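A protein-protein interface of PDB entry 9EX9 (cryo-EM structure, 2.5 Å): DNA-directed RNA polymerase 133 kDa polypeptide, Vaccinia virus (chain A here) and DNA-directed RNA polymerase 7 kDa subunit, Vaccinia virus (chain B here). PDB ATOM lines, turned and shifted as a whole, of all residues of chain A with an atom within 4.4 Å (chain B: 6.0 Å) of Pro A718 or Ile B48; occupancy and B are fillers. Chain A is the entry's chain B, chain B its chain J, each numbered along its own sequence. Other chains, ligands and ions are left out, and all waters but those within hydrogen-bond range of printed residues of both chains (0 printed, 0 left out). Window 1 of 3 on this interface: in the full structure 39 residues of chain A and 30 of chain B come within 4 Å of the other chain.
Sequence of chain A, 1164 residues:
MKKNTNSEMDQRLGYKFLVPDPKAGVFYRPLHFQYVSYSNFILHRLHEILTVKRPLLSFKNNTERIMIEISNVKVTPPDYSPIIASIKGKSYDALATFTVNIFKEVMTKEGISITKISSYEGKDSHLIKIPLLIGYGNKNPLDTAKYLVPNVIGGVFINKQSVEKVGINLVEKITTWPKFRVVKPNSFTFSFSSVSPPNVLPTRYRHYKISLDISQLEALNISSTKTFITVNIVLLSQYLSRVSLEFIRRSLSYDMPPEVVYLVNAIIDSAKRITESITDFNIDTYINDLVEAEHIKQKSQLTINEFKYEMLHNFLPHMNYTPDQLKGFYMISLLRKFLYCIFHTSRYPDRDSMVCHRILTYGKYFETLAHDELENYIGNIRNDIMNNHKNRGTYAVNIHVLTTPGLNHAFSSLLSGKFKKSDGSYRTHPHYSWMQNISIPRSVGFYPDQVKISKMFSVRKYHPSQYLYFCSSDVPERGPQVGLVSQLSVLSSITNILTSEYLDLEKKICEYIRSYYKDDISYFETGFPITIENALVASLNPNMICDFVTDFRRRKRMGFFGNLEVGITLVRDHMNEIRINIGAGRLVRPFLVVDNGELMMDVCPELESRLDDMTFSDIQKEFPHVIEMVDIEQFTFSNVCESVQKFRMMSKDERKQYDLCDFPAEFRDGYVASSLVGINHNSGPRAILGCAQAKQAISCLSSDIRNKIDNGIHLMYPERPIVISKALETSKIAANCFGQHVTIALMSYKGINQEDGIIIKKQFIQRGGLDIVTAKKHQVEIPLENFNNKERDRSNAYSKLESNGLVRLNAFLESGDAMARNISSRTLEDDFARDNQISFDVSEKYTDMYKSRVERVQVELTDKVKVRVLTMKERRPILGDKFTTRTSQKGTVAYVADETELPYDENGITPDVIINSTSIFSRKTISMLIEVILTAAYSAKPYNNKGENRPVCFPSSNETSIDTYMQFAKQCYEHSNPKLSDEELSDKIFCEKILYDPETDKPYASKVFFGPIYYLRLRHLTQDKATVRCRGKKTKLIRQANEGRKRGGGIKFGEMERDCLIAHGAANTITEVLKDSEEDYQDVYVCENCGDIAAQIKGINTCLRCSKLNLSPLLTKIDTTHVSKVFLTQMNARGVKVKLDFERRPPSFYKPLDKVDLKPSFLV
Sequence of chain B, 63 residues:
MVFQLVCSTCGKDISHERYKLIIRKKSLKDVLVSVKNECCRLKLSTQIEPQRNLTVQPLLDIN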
ATOM      1  N   CYS A 700      16.923   9.050  -5.199  1.00  0.00           N
ATOM      2  CA  CYS A 700      15.864   8.101  -5.537  1.00  0.00           C
ATOM      3  C   CYS A 700      14.683   8.905  -6.061  1.00  0.00           C
ATOM      4  O   CYS A 700      13.815   9.346  -5.310  1.00  0.00           O
ATOM      5  CB  CYS A 700      15.479   7.264  -4.326  1.00  0.00           C
ATOM      6  SG  CYS A 700      16.803   6.233  -3.698  1.00  0.00           S
ATOM      7  N   LEU A 715      19.604   7.060  -8.559  1.00  0.00           N
ATOM      8  CA  LEU A 715      20.750   6.553  -7.813  1.00  0.00           C
ATOM      9  C   LEU A 715      20.549   5.079  -7.480  1.00  0.00           C
ATOM     10  O   LEU A 715      19.476   4.675  -7.027  1.00  0.00           O
ATOM     11  CB  LEU A 715      20.926   7.369  -6.534  1.00  0.00           C
ATOM     12  CG  LEU A 715      22.113   7.094  -5.614  1.00  0.00           C
ATOM     13  CD1 LEU A 715      23.406   7.612  -6.207  1.00  0.00           C
ATOM     14  CD2 LEU A 715      21.853   7.731  -4.268  1.00  0.00           C
ATOM     15  N   MET A 716      21.595   4.275  -7.683  1.00  0.00           N
ATOM     16  CA  MET A 716      21.418   2.827  -7.765  1.00  0.00           C
ATOM     17  C   MET A 716      21.464   2.120  -6.414  1.00  0.00           C
ATOM     18  O   MET A 716      20.641   1.236  -6.163  1.00  0.00           O
ATOM     19  CB  MET A 716      22.465   2.221  -8.701  1.00  0.00           C
ATOM     20  CG  MET A 716      22.112   2.373 -10.169  1.00  0.00           C
ATOM     21  SD  MET A 716      23.232   1.533 -11.296  1.00  0.00           S
ATOM     22  CE  MET A 716      22.936  -0.172 -10.864  1.00  0.00           C
ATOM     23  N   TYR A 717      22.408   2.466  -5.541  1.00  0.00           N
ATOM     24  CA  TYR A 717      22.546   1.820  -4.233  1.00  0.00           C
ATOM     25  C   TYR A 717      22.554   2.902  -3.165  1.00  0.00           C
ATOM     26  O   TYR A 717      23.609   3.259  -2.629  1.00  0.00           O
ATOM     27  CB  TYR A 717      23.807   0.959  -4.162  1.00  0.00           C
ATOM     28  CG  TYR A 717      23.827  -0.175  -5.161  1.00  0.00           C
ATOM     29  CD1 TYR A 717      23.124  -1.343  -4.928  1.00  0.00           C
ATOM     30  CD2 TYR A 717      24.552  -0.074  -6.337  1.00  0.00           C
ATOM     31  CE1 TYR A 717      23.138  -2.373  -5.838  1.00  0.00           C
ATOM     32  CE2 TYR A 717      24.571  -1.100  -7.249  1.00  0.00           C
ATOM     33  CZ  TYR A 717      23.863  -2.244  -6.995  1.00  0.00           C
ATOM     34  OH  TYR A 717      23.881  -3.269  -7.904  1.00  0.00           O
ATOM     35  N   PRO A 718      21.387   3.440  -2.824  1.00  0.00           N
ATOM     36  CA  PRO A 718      21.340   4.638  -1.985  1.00  0.00           C
ATOM     37  C   PRO A 718      21.682   4.360  -0.530  1.00  0.00           C
ATOM     38  O   PRO A 718      21.594   3.235  -0.035  1.00  0.00           O
ATOM     39  CB  PRO A 718      19.889   5.098  -2.129  1.00  0.00           C
ATOM     40  CG  PRO A 718      19.144   3.847  -2.376  1.00  0.00           C
ATOM     41  CD  PRO A 718      20.040   2.980  -3.197  1.00  0.00           C
ATOM     42  N   GLU A 719      22.079   5.429   0.156  1.00  0.00           N
ATOM     43  CA  GLU A 719      22.364   5.408   1.581  1.00  0.00           C
ATOM     44  C   GLU A 719      21.696   6.596   2.250  1.00  0.00           C
ATOM     45  O   GLU A 719      21.583   7.676   1.666  1.00  0.00           O
ATOM     46  CB  GLU A 719      23.861   5.456   1.865  1.00  0.00           C
ATOM     47  CG  GLU A 719      24.576   4.164   1.593  1.00  0.00           C
ATOM     48  CD  GLU A 719      25.999   4.184   2.077  1.00  0.00           C
ATOM     49  OE1 GLU A 719      26.221   4.488   3.268  1.00  0.00           O
ATOM     50  OE2 GLU A 719      26.904   3.903   1.266  1.00  0.00           O
ATOM     51  N   ARG A 720      21.279   6.390   3.493  1.00  0.00           N
ATOM     52  CA  ARG A 720      20.565   7.409   4.247  1.00  0.00           C
ATOM     53  C   ARG A 720      21.550   8.214   5.084  1.00  0.00           C
ATOM     54  O   ARG A 720      22.286   7.624   5.882  1.00  0.00           O
ATOM     55  CB  ARG A 720      19.533   6.759   5.143  1.00  0.00           C
ATOM     56  CG  ARG A 720      18.581   7.723   5.794  1.00  0.00           C
ATOM     57  CD  ARG A 720      17.639   7.011   6.739  1.00  0.00           C
ATOM     58  NE  ARG A 720      18.356   6.356   7.827  1.00  0.00           N
ATOM     59  CZ  ARG A 720      18.736   5.085   7.825  1.00  0.00           C
ATOM     60  NH1 ARG A 720      18.478   4.284   6.805  1.00  0.00           N
ATOM     61  NH2 ARG A 720      19.394   4.606   8.875  1.00  0.00           N
ATOM     62  N   ALA A 735      15.000  10.254   3.875  1.00  0.00           N
ATOM     63  CA  ALA A 735      14.607   8.878   3.606  1.00  0.00           C
ATOM     64  C   ALA A 735      14.650   8.525   2.129  1.00  0.00           C
ATOM     65  O   ALA A 735      14.483   7.350   1.794  1.00  0.00           O
ATOM     66  CB  ALA A 735      13.203   8.617   4.144  1.00  0.00           C
ATOM     67  N   CYS A 737      17.322   9.811   0.084  1.00  0.00           N
ATOM     68  CA  CYS A 737      18.737   9.612  -0.214  1.00  0.00           C
ATOM     69  C   CYS A 737      19.223  10.472  -1.370  1.00  0.00           C
ATOM     70  O   CYS A 737      18.542  10.584  -2.390  1.00  0.00           O
ATOM     71  CB  CYS A 737      18.996   8.140  -0.524  1.00  0.00           C
ATOM     72  SG  CYS A 737      18.311   7.013   0.695  1.00  0.00           S
ATOM     73  N   VAL B   2      20.720  -2.828   0.792  1.00  0.00           N
ATOM     74  CA  VAL B   2      20.436  -4.202   1.168  1.00  0.00           C
ATOM     75  C   VAL B   2      20.733  -5.134   0.000  1.00  0.00           C
ATOM     76  O   VAL B   2      20.405  -6.313   0.029  1.00  0.00           O
ATOM     77  CB  VAL B   2      18.990  -4.340   1.641  1.00  0.00           C
ATOM     78  CG1 VAL B   2      18.658  -5.780   1.981  1.00  0.00           C
ATOM     79  CG2 VAL B   2      18.762  -3.446   2.838  1.00  0.00           C
ATOM     80  N   PHE B   3      21.400  -4.597  -1.016  1.00  0.00           N
ATOM     81  CA  PHE B   3      21.560  -5.261  -2.300  1.00  0.00           C
ATOM     82  C   PHE B   3      22.993  -5.689  -2.573  1.00  0.00           C
ATOM     83  O   PHE B   3      23.234  -6.848  -2.918  1.00  0.00           O
ATOM     84  CB  PHE B   3      21.069  -4.317  -3.403  1.00  0.00           C
ATOM     85  CG  PHE B   3      20.224  -4.980  -4.446  1.00  0.00           C
ATOM     86  CD1 PHE B   3      18.885  -5.201  -4.229  1.00  0.00           C
ATOM     87  CD2 PHE B   3      20.768  -5.359  -5.659  1.00  0.00           C
ATOM     88  CE1 PHE B   3      18.110  -5.801  -5.195  1.00  0.00           C
ATOM     89  CE2 PHE B   3      19.995  -5.958  -6.622  1.00  0.00           C
ATOM     90  CZ  PHE B   3      18.667  -6.176  -6.391  1.00  0.00           C
ATOM     91  N   ARG B  18      24.140  -8.779   6.844  1.00  0.00           N
ATOM     92  CA  ARG B  18      22.944  -8.172   6.276  1.00  0.00           C
ATOM     93  C   ARG B  18      21.721  -9.054   6.483  1.00  0.00           C
ATOM     94  O   ARG B  18      20.640  -8.557   6.814  1.00  0.00           O
ATOM     95  CB  ARG B  18      23.154  -7.896   4.794  1.00  0.00           C
ATOM     96  CG  ARG B  18      22.172  -6.920   4.237  1.00  0.00           C
ATOM     97  CD  ARG B  18      22.409  -6.703   2.773  1.00  0.00           C
ATOM     98  NE  ARG B  18      23.596  -5.912   2.472  1.00  0.00           N
ATOM     99  CZ  ARG B  18      23.752  -4.628   2.763  1.00  0.00           C
ATOM    100  NH1 ARG B  18      22.859  -3.965   3.474  1.00  0.00           N
ATOM    101  NH2 ARG B  18      24.834  -3.993   2.332  1.00  0.00           N
ATOM    102  N   THR B  46      23.636   2.298   7.248  1.00  0.00           N
ATOM    103  CA  THR B  46      22.947   3.342   6.499  1.00  0.00           C
ATOM    104  C   THR B  46      22.384   2.913   5.150  1.00  0.00           C
ATOM    105  O   THR B  46      21.775   3.743   4.471  1.00  0.00           O
ATOM    106  CB  THR B  46      23.881   4.538   6.272  1.00  0.00           C
ATOM    107  OG1 THR B  46      24.982   4.144   5.448  1.00  0.00           O
ATOM    108  CG2 THR B  46      24.404   5.061   7.591  1.00  0.00           C
ATOM    109  N   GLN B  47      22.547   1.661   4.739  1.00  0.00           N
ATOM    110  CA  GLN B  47      22.094   1.238   3.420  1.00  0.00           C
ATOM    111  C   GLN B  47      20.668   0.715   3.476  1.00  0.00           C
ATOM    112  O   GLN B  47      20.288   0.004   4.408  1.00  0.00           O
ATOM    113  CB  GLN B  47      23.018   0.166   2.846  1.00  0.00           C
ATOM    114  CG  GLN B  47      24.128   0.730   1.988  1.00  0.00           C
ATOM    115  CD  GLN B  47      24.997  -0.341   1.381  1.00  0.00           C
ATOM    116  OE1 GLN B  47      24.839  -1.521   1.673  1.00  0.00           O
ATOM    117  NE2 GLN B  47      25.922   0.066   0.529  1.00  0.00           N
ATOM    118  N   ILE B  48      19.884   1.070   2.456  1.00  0.00           N
ATOM    119  CA  ILE B  48      18.470   0.733   2.379  1.00  0.00           C
ATOM    120  C   ILE B  48      18.158   0.195   0.993  1.00  0.00           C
ATOM    121  O   ILE B  48      18.893   0.424   0.031  1.00  0.00           O
ATOM    122  CB  ILE B  48      17.569   1.949   2.671  1.00  0.00           C
ATOM    123  CG1 ILE B  48      17.836   3.060   1.656  1.00  0.00           C
ATOM    124  CG2 ILE B  48      17.799   2.458   4.077  1.00  0.00           C
ATOM    125  CD1 ILE B  48      16.851   4.175   1.721  1.00  0.00           C
ATOM    126  N   GLU B  49      17.038  -0.513   0.898  1.00  0.00           N
ATOM    127  CA  GLU B  49      16.459  -0.868  -0.391  1.00  0.00           C
ATOM    128  C   GLU B  49      15.335   0.100  -0.723  1.00  0.00           C
ATOM    129  O   GLU B  49      14.418   0.269   0.091  1.00  0.00           O
ATOM    130  CB  GLU B  49      15.928  -2.297  -0.369  1.00  0.00           C
ATOM    131  CG  GLU B  49      16.549  -3.197  -1.424  1.00  0.00           C
ATOM    132  CD  GLU B  49      16.191  -4.653  -1.237  1.00  0.00           C
ATOM    133  OE1 GLU B  49      15.733  -5.014  -0.137  1.00  0.00           O
ATOM    134  OE2 GLU B  49      16.365  -5.442  -2.186  1.00  0.00           O
ATOM    135  N   PRO B  50      15.355   0.757  -1.879  1.00  0.00           N
ATOM    136  CA  PRO B  50      14.395   1.837  -2.126  1.00  0.00           C
ATOM    137  C   PRO B  50      12.963   1.338  -2.227  1.00  0.00           C
ATOM    138  O   PRO B  50      12.700   0.171  -2.520  1.00  0.00           O
ATOM    139  CB  PRO B  50      14.870   2.430  -3.455  1.00  0.00           C
ATOM    140  CG  PRO B  50      15.582   1.328  -4.125  1.00  0.00           C
ATOM    141  CD  PRO B  50      16.228   0.527  -3.041  1.00  0.00           C
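The backbone carbonyl oxygen of Thr B46 is in hydrogen-bond range of the backbone NH of Arg A720, 2.9 Å away. The side-chain carboxylate (OE1) of Glu A719 sits at hydrogen-bond distance from the side-chain hydroxyl (OG1) of Thr B46 (2.5 Å).
Phe B3 touches Tyr A717. N of Ile B48 touches O of Pro A718, 3.7 Å away. CG of Glu A719 touches CG of Gln B47, at 3.5 Å. NH1 of Arg A720 touches CG2 of Ile B48 (3.4 Å). CD1 of Ile B48 touches O of Ala A735, at 3.96 Å. Cys A737 touches Ile B48 (SG to CD1, 3.4 Å).
OE1 of Gln B47 lies within hydrogen-bond range of NH2 of Arg B18 (2.6 Å). The backbone carbonyl oxygen (O) of Glu A719 sits close to the side-chain sulfur (SG) of Cys A737 (3.5 Å).
Of the 8 printed residues of chain B, 4 touch a printed residue of chain A. Along chain B the printed residues that touch a printed residue of chain A span positions 3 to 48. Of the 9 printed residues of chain A, 6 touch a printed residue of chain B. Printed residues of chain A that touch a printed residue of chain B: Tyr A717, Pro A718, Glu A719, Arg A720, Ala A735 and Cys A737. Hydrophobic or aromatic side chains of chain A that line the printed part of chain B: Tyr A717. Among the printed residues, 8 pairs touch across the chains. Among the printed residues, no Asp or Glu carboxylate lies within 4 Å of a Lys or Arg side-chain nitrogen of the other chain.
Of the printed residues of chain B, Tyr A717 touches Phe B3. Of chain B, only Ile B48 comes within 4 Å of Pro A718. Of the printed residues of chain B, Glu A719 touches Thr B46 and Gln B47. Printed residues of chain B within 4 Å of Arg A720: Thr B46 and Ile B48. Printed residues of chain A within 4 Å of Gln B47: Glu A719 (3.5 Å). Of the printed residues of chain A, Ile B48 touches Pro A718, Arg A720, Ala A735 and Cys A737. The nearest residue of chain B that does not touch Pro A718 is Gln B47 (4.02 Å). The nearest printed residue of chain B that does not touch Ala A735 is Pro B50 (6.8 Å).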
